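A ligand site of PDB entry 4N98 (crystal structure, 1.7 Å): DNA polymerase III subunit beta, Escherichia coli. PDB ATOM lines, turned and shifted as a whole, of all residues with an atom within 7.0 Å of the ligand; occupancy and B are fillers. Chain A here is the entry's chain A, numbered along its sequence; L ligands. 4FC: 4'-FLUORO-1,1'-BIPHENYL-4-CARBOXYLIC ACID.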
ATOM      1  N   ARG A 152     -21.728  19.327  -0.277  1.00  0.00           N
ATOM      2  CA  ARG A 152     -22.528  20.527  -0.212  1.00  0.00           C
ATOM      3  C   ARG A 152     -23.857  20.119  -0.782  1.00  0.00           C
ATOM      4  O   ARG A 152     -24.068  20.169  -1.985  1.00  0.00           O
ATOM      5  CB  ARG A 152     -21.933  21.680  -1.025  1.00  0.00           C
ATOM      6  CG  ARG A 152     -20.511  22.044  -0.644  1.00  0.00           C
ATOM      7  CD  ARG A 152     -19.541  21.623  -1.720  1.00  0.00           C
ATOM      8  NE  ARG A 152     -18.921  22.750  -2.374  1.00  0.00           N
ATOM      9  CZ  ARG A 152     -18.231  22.708  -3.507  1.00  0.00           C
ATOM     10  NH1 ARG A 152     -18.062  21.568  -4.187  1.00  0.00           N
ATOM     11  NH2 ARG A 152     -17.706  23.831  -3.973  1.00  0.00           N
ATOM     12  N   TYR A 154     -26.638  21.375  -0.932  1.00  0.00           N
ATOM     13  CA  TYR A 154     -27.390  22.429  -1.644  1.00  0.00           C
ATOM     14  C   TYR A 154     -27.082  22.466  -3.163  1.00  0.00           C
ATOM     15  O   TYR A 154     -27.835  23.060  -3.933  1.00  0.00           O
ATOM     16  CB  TYR A 154     -27.183  23.820  -0.983  1.00  0.00           C
ATOM     17  CG  TYR A 154     -25.744  24.308  -0.837  1.00  0.00           C
ATOM     18  CD1 TYR A 154     -25.095  24.933  -1.891  1.00  0.00           C
ATOM     19  CD2 TYR A 154     -25.049  24.156   0.362  1.00  0.00           C
ATOM     20  CE1 TYR A 154     -23.789  25.375  -1.771  1.00  0.00           C
ATOM     21  CE2 TYR A 154     -23.740  24.606   0.497  1.00  0.00           C
ATOM     22  CZ  TYR A 154     -23.113  25.211  -0.570  1.00  0.00           C
ATOM     23  OH  TYR A 154     -21.820  25.650  -0.446  1.00  0.00           O
ATOM     24  N   LEU A 155     -25.990  21.812  -3.563  1.00  0.00           N
ATOM     25  CA  LEU A 155     -25.596  21.736  -4.975  1.00  0.00           C
ATOM     26  C   LEU A 155     -26.179  20.516  -5.691  1.00  0.00           C
ATOM     27  O   LEU A 155     -26.089  20.458  -6.930  1.00  0.00           O
ATOM     28  CB  LEU A 155     -24.069  21.686  -5.091  1.00  0.00           C
ATOM     29  CG  LEU A 155     -23.254  22.909  -4.638  1.00  0.00           C
ATOM     30  CD1 LEU A 155     -21.807  22.695  -5.017  1.00  0.00           C
ATOM     31  CD2 LEU A 155     -23.780  24.203  -5.247  1.00  0.00           C
ATOM     32  N   THR A 172     -25.147  24.184 -10.448  1.00  0.00           N
ATOM     33  CA  THR A 172     -23.699  24.187 -10.401  1.00  0.00           C
ATOM     34  C   THR A 172     -23.197  23.115  -9.475  1.00  0.00           C
ATOM     35  O   THR A 172     -23.900  22.733  -8.532  1.00  0.00           O
ATOM     36  CB  THR A 172     -23.130  25.549  -9.956  1.00  0.00           C
ATOM     37  OG1 THR A 172     -21.690  25.549 -10.042  1.00  0.00           O
ATOM     38  CG2 THR A 172     -23.533  25.888  -8.543  1.00  0.00           C
ATOM     39  N   ASP A 173     -22.004  22.605  -9.767  1.00  0.00           N
ATOM     40  CA  ASP A 173     -21.358  21.578  -8.980  1.00  0.00           C
ATOM     41  C   ASP A 173     -20.062  22.106  -8.365  1.00  0.00           C
ATOM     42  O   ASP A 173     -19.232  21.325  -7.907  1.00  0.00           O
ATOM     43  CB  ASP A 173     -21.069  20.343  -9.828  1.00  0.00           C
ATOM     44  CG  ASP A 173     -20.155  20.622 -10.996  1.00  0.00           C
ATOM     45  OD1 ASP A 173     -19.633  21.757 -11.135  1.00  0.00           O
ATOM     46  OD2 ASP A 173     -19.962  19.681 -11.799  1.00  0.00           O
ATOM     47  N   GLY A 174     -19.891  23.419  -8.370  1.00  0.00           N
ATOM     48  CA  GLY A 174     -18.710  24.031  -7.805  1.00  0.00           C
ATOM     49  C   GLY A 174     -17.560  24.196  -8.799  1.00  0.00           C
ATOM     50  O   GLY A 174     -16.557  24.798  -8.454  1.00  0.00           O
ATOM     51  N   HIS A 175     -17.707  23.621  -9.995  1.00  0.00           N
ATOM     52  CA  HIS A 175     -16.665  23.686 -11.032  1.00  0.00           C
ATOM     53  C   HIS A 175     -17.161  24.330 -12.320  1.00  0.00           C
ATOM     54  O   HIS A 175     -16.408  25.042 -13.005  1.00  0.00           O
ATOM     55  CB  HIS A 175     -16.152  22.294 -11.332  1.00  0.00           C
ATOM     56  CG  HIS A 175     -15.623  21.577 -10.124  1.00  0.00           C
ATOM     57  ND1 HIS A 175     -14.446  21.927  -9.505  1.00  0.00           N
ATOM     58  CD2 HIS A 175     -16.134  20.545  -9.406  1.00  0.00           C
ATOM     59  CE1 HIS A 175     -14.251  21.141  -8.455  1.00  0.00           C
ATOM     60  NE2 HIS A 175     -15.251  20.286  -8.388  1.00  0.00           N
ATOM     61  N   ARG A 176     -18.424  24.099 -12.638  1.00  0.00           N
ATOM     62  CA  ARG A 176     -19.061  24.710 -13.794  1.00  0.00           C
ATOM     63  C   ARG A 176     -20.491  25.045 -13.380  1.00  0.00           C
ATOM     64  O   ARG A 176     -21.025  24.446 -12.450  1.00  0.00           O
ATOM     65  CB  ARG A 176     -19.013  23.770 -14.997  1.00  0.00           C
ATOM     66  CG  ARG A 176     -19.242  22.289 -14.703  1.00  0.00           C
ATOM     67  CD  ARG A 176     -20.722  21.921 -14.654  1.00  0.00           C
ATOM     68  NE  ARG A 176     -20.898  20.485 -14.470  1.00  0.00           N
ATOM     69  CZ  ARG A 176     -20.842  19.568 -15.430  1.00  0.00           C
ATOM     70  NH1 ARG A 176     -20.656  19.902 -16.706  1.00  0.00           N
ATOM     71  NH2 ARG A 176     -20.988  18.287 -15.113  1.00  0.00           N
ATOM     72  N   LEU A 177     -21.080  26.016 -14.052  1.00  0.00           N
ATOM     73  CA  LEU A 177     -22.400  26.519 -13.682  1.00  0.00           C
ATOM     74  C   LEU A 177     -23.236  26.766 -14.936  1.00  0.00           C
ATOM     75  O   LEU A 177     -22.713  27.139 -15.974  1.00  0.00           O
ATOM     76  CB  LEU A 177     -22.254  27.789 -12.826  1.00  0.00           C
ATOM     77  CG  LEU A 177     -23.518  28.613 -12.488  1.00  0.00           C
ATOM     78  CD1 LEU A 177     -23.377  29.314 -11.146  1.00  0.00           C
ATOM     79  CD2 LEU A 177     -23.878  29.600 -13.599  1.00  0.00           C
ATOM     80  N   ARG A 240     -27.498  27.555   1.599  1.00  0.00           N
ATOM     81  CA  ARG A 240     -27.225  28.822   0.934  1.00  0.00           C
ATOM     82  C   ARG A 240     -26.616  28.574  -0.449  1.00  0.00           C
ATOM     83  O   ARG A 240     -25.423  28.325  -0.585  1.00  0.00           O
ATOM     84  CB  ARG A 240     -26.300  29.663   1.839  1.00  0.00           C
ATOM     85  CG  ARG A 240     -27.052  30.308   3.001  1.00  0.00           C
ATOM     86  CD  ARG A 240     -26.360  30.291   4.361  1.00  0.00           C
ATOM     87  NE  ARG A 240     -24.892  30.340   4.363  1.00  0.00           N
ATOM     88  CZ  ARG A 240     -24.144  31.321   3.878  1.00  0.00           C
ATOM     89  NH1 ARG A 240     -24.706  32.370   3.286  1.00  0.00           N
ATOM     90  NH2 ARG A 240     -22.810  31.251   3.961  1.00  0.00           N
ATOM     91  N   PHE A 241     -27.470  28.624  -1.484  1.00  0.00           N
ATOM     92  CA  PHE A 241     -27.048  28.365  -2.862  1.00  0.00           C
ATOM     93  C   PHE A 241     -26.150  29.505  -3.315  1.00  0.00           C
ATOM     94  O   PHE A 241     -26.400  30.674  -2.975  1.00  0.00           O
ATOM     95  CB  PHE A 241     -28.261  28.222  -3.793  1.00  0.00           C
ATOM     96  CG  PHE A 241     -27.990  27.461  -5.084  1.00  0.00           C
ATOM     97  CD1 PHE A 241     -28.072  26.088  -5.116  1.00  0.00           C
ATOM     98  CD2 PHE A 241     -27.665  28.130  -6.262  1.00  0.00           C
ATOM     99  CE1 PHE A 241     -27.822  25.370  -6.288  1.00  0.00           C
ATOM    100  CE2 PHE A 241     -27.408  27.445  -7.432  1.00  0.00           C
ATOM    101  CZ  PHE A 241     -27.492  26.059  -7.457  1.00  0.00           C
ATOM    102  N   PRO A 242     -25.098  29.203  -4.092  1.00  0.00           N
ATOM    103  CA  PRO A 242     -24.266  30.303  -4.599  1.00  0.00           C
ATOM    104  C   PRO A 242     -25.027  31.272  -5.489  1.00  0.00           C
ATOM    105  O   PRO A 242     -26.065  30.930  -6.043  1.00  0.00           O
ATOM    106  CB  PRO A 242     -23.195  29.576  -5.435  1.00  0.00           C
ATOM    107  CG  PRO A 242     -23.817  28.288  -5.790  1.00  0.00           C
ATOM    108  CD  PRO A 242     -24.625  27.908  -4.590  1.00  0.00           C
ATOM    109  N   ASP A 243     -24.470  32.471  -5.632  1.00  0.00           N
ATOM    110  CA  ASP A 243     -25.066  33.543  -6.393  1.00  0.00           C
ATOM    111  C   ASP A 243     -24.447  33.557  -7.783  1.00  0.00           C
ATOM    112  O   ASP A 243     -23.263  33.852  -7.922  1.00  0.00           O
ATOM    113  CB  ASP A 243     -24.777  34.871  -5.668  1.00  0.00           C
ATOM    114  CG  ASP A 243     -25.233  36.092  -6.435  1.00  0.00           C
ATOM    115  OD1 ASP A 243     -25.834  35.971  -7.520  1.00  0.00           O
ATOM    116  OD2 ASP A 243     -24.994  37.207  -5.916  1.00  0.00           O
ATOM    117  N   ARG A 246     -22.076  36.191  -9.073  1.00  0.00           N
ATOM    118  CA  ARG A 246     -20.667  36.116  -8.621  1.00  0.00           C
ATOM    119  C   ARG A 246     -19.814  35.170  -9.442  1.00  0.00           C
ATOM    120  O   ARG A 246     -18.590  35.252  -9.435  1.00  0.00           O
ATOM    121  CB  ARG A 246     -20.601  35.629  -7.176  1.00  0.00           C
ATOM    122  CG  ARG A 246     -21.284  36.537  -6.182  1.00  0.00           C
ATOM    123  CD  ARG A 246     -20.417  37.748  -5.869  1.00  0.00           C
ATOM    124  NE  ARG A 246     -21.182  38.979  -5.963  1.00  0.00           N
ATOM    125  CZ  ARG A 246     -20.672  40.186  -5.724  1.00  0.00           C
ATOM    126  NH1 ARG A 246     -19.392  40.333  -5.374  1.00  0.00           N
ATOM    127  NH2 ARG A 246     -21.455  41.247  -5.854  1.00  0.00           N
ATOM    128  N   VAL A 247     -20.463  34.206 -10.098  1.00  0.00           N
ATOM    129  CA  VAL A 247     -19.758  33.226 -10.883  1.00  0.00           C
ATOM    130  C   VAL A 247     -19.572  33.733 -12.310  1.00  0.00           C
ATOM    131  O   VAL A 247     -18.559  33.445 -12.950  1.00  0.00           O
ATOM    132  CB  VAL A 247     -20.489  31.856 -10.866  1.00  0.00           C
ATOM    133  CG1 VAL A 247     -19.810  30.878 -11.811  1.00  0.00           C
ATOM    134  CG2 VAL A 247     -20.517  31.293  -9.445  1.00  0.00           C
ATOM    135  N   LEU A 248     -20.549  34.507 -12.804  1.00  0.00           N
ATOM    136  CA  LEU A 248     -20.429  35.120 -14.129  1.00  0.00           C
ATOM    137  C   LEU A 248     -19.240  36.070 -14.119  1.00  0.00           C
ATOM    138  O   LEU A 248     -19.130  36.900 -13.220  1.00  0.00           O
ATOM    139  CB  LEU A 248     -21.687  35.922 -14.519  1.00  0.00           C
ATOM    140  CG  LEU A 248     -23.011  35.195 -14.800  1.00  0.00           C
ATOM    141  CD1 LEU A 248     -24.138  36.179 -15.074  1.00  0.00           C
ATOM    142  CD2 LEU A 248     -22.870  34.224 -15.952  1.00  0.00           C
ATOM    143  N   SER A 346     -12.493  32.252 -15.246  1.00  0.00           N
ATOM    144  CA  SER A 346     -13.484  31.382 -15.891  1.00  0.00           C
ATOM    145  C   SER A 346     -13.821  31.861 -17.280  1.00  0.00           C
ATOM    146  O   SER A 346     -13.582  32.999 -17.620  1.00  0.00           O
ATOM    147  CB  SER A 346     -14.772  31.319 -15.061  1.00  0.00           C
ATOM    148  OG  SER A 346     -14.518  30.608 -13.849  1.00  0.00           O
ATOM    149  N   VAL A 347     -14.381  30.962 -18.088  1.00  0.00           N
ATOM    150  CA  VAL A 347     -14.956  31.360 -19.377  1.00  0.00           C
ATOM    151  C   VAL A 347     -16.475  31.283 -19.297  1.00  0.00           C
ATOM    152  O   VAL A 347     -17.014  30.421 -18.620  1.00  0.00           O
ATOM    153  CB  VAL A 347     -14.466  30.458 -20.550  1.00  0.00           C
ATOM    154  CG1 VAL A 347     -14.883  29.007 -20.375  1.00  0.00           C
ATOM    155  CG2 VAL A 347     -14.974  30.981 -21.886  1.00  0.00           C
ATOM    156  N   VAL A 360     -20.775  28.817 -17.276  1.00  0.00           N
ATOM    157  CA  VAL A 360     -19.503  29.272 -16.778  1.00  0.00           C
ATOM    158  C   VAL A 360     -18.681  28.055 -16.408  1.00  0.00           C
ATOM    159  O   VAL A 360     -19.158  27.172 -15.671  1.00  0.00           O
ATOM    160  CB  VAL A 360     -19.637  30.199 -15.567  1.00  0.00           C
ATOM    161  CG1 VAL A 360     -18.267  30.640 -15.059  1.00  0.00           C
ATOM    162  CG2 VAL A 360     -20.486  31.409 -15.929  1.00  0.00           C
ATOM    163  N   VAL A 361     -17.466  27.975 -16.952  1.00  0.00           N
ATOM    164  CA  VAL A 361     -16.545  26.898 -16.635  1.00  0.00           C
ATOM    165  C   VAL A 361     -15.259  27.460 -16.023  1.00  0.00           C
ATOM    166  O   VAL A 361     -14.667  28.393 -16.562  1.00  0.00           O
ATOM    167  CB  VAL A 361     -16.225  26.069 -17.900  1.00  0.00           C
ATOM    168  CG1 VAL A 361     -15.294  24.906 -17.575  1.00  0.00           C
ATOM    169  CG2 VAL A 361     -17.512  25.566 -18.541  1.00  0.00           C
ATOM    170  N   MET A 362     -14.834  26.901 -14.890  1.00  0.00           N
ATOM    171  CA  MET A 362     -13.586  27.320 -14.253  1.00  0.00           C
ATOM    172  C   MET A 362     -12.382  26.843 -15.060  1.00  0.00           C
ATOM    173  O   MET A 362     -12.426  25.808 -15.697  1.00  0.00           O
ATOM    174  CB  MET A 362     -13.485  26.783 -12.814  1.00  0.00           C
ATOM    175  CG  MET A 362     -14.342  27.527 -11.807  1.00  0.00           C
ATOM    176  SD  MET A 362     -14.051  29.315 -11.776  1.00  0.00           S
ATOM    177  CE  MET A 362     -12.670  29.428 -10.643  1.00  0.00           C
ATOM    178  N   PRO A 363     -11.290  27.639 -15.054  1.00  0.00           N
ATOM    179  CA  PRO A 363     -10.079  27.195 -15.735  1.00  0.00           C
ATOM    180  C   PRO A 363      -9.377  26.128 -14.897  1.00  0.00           C
ATOM    181  O   PRO A 363      -9.683  25.981 -13.722  1.00  0.00           O
ATOM    182  CB  PRO A 363      -9.253  28.480 -15.818  1.00  0.00           C
ATOM    183  CG  PRO A 363      -9.625  29.215 -14.581  1.00  0.00           C
ATOM    184  CD  PRO A 363     -11.040  28.840 -14.246  1.00  0.00           C
HETATM  185  C1  4FC L   1     -18.690  27.409 -10.975  1.00  0.00           C
HETATM  186  C2  4FC L   1     -17.635  28.236 -11.291  1.00  0.00           C
HETATM  187  C3  4FC L   1     -16.896  28.826 -10.268  1.00  0.00           C
HETATM  188  C4  4FC L   1     -17.210  28.602  -8.936  1.00  0.00           C
HETATM  189  C5  4FC L   1     -18.283  27.789  -8.616  1.00  0.00           C
HETATM  190  C6  4FC L   1     -19.017  27.182  -9.638  1.00  0.00           C
HETATM  191  C7  4FC L   1     -17.618  27.213  -6.360  1.00  0.00           C
HETATM  192  C8  4FC L   1     -18.616  27.517  -7.289  1.00  0.00           C
HETATM  193  C9  4FC L   1     -19.961  27.497  -6.888  1.00  0.00           C
HETATM  194  C10 4FC L   1     -20.275  27.200  -5.572  1.00  0.00           C
HETATM  195  C11 4FC L   1     -19.296  26.909  -4.639  1.00  0.00           C
HETATM  196  C12 4FC L   1     -17.956  26.922  -5.042  1.00  0.00           C
HETATM  197  F1  4FC L   1     -17.302  28.466 -12.604  1.00  0.00           F
HETATM  198  C13 4FC L   1     -19.663  26.603  -3.328  1.00  0.00           C
HETATM  199  O1  4FC L   1     -20.845  26.779  -2.943  1.00  0.00           O
HETATM  200  O2  4FC L   1     -18.828  26.094  -2.537  1.00  0.00           O
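O2 of the ligand is in salt-bridge range of NH2 of Arg 152, 2.9 Å away. The side-chain hydroxyl (OH) of Tyr 154 lies within hydrogen-bond range of an oxygen (O1) of the ligand.
The side-chain hydroxyl (OG1) of Thr 172 lies within hydrogen-bond range of the backbone NH (N) of Gly 174 (3.3 Å). The backbone carbonyl oxygen of Arg 176 is in hydrogen-bond range of the side-chain hydroxyl of Thr 172 (2.7 Å). The backbone NH (N) of Met 362 is in hydrogen-bond range of the backbone carbonyl oxygen (O) of His 175 (3.1 Å). The side-chain hydroxyl (OG) of Ser 346 sits at hydrogen-bond distance from the side-chain sulfur (SD) of Met 362 (2.5 Å). The backbone carbonyl oxygen (O) of Val 360 sits at hydrogen-bond distance from the backbone NH (N) of Leu 177 (2.8 Å). The side-chain carboxylate (OD1) of Asp 173 lies within hydrogen-bond range of the backbone NH (N) of His 175. The guanidinium group (NE) of Arg 176 lies within salt-bridge range of the side-chain carboxylate (OD2) of Asp 173 (2.9 Å).
SD of Met 362 lies close to F1 of the ligand (3.5 Å). Thr 172 touches the ligand. O of Gly 174 touches C7 of the ligand, 3.4 Å away. O of His 175 touches F1 of the ligand, 3.6 Å away. Arg 176 touches the ligand. Pro 242 touches the ligand (CG to C10, 3.7 Å). Val 247 touches the ligand. OG of Ser 346 touches F1 of the ligand, 3.7 Å away. Val 360 touches the ligand (CG1 to F1, 3.4 Å). Hydrophobic or aromatic side chains that line the ligand: Tyr 154, Pro 242, Val 247, Val 360 and Met 362. Of the 22 residues printed, 11 come within 4 Å of the ligand.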
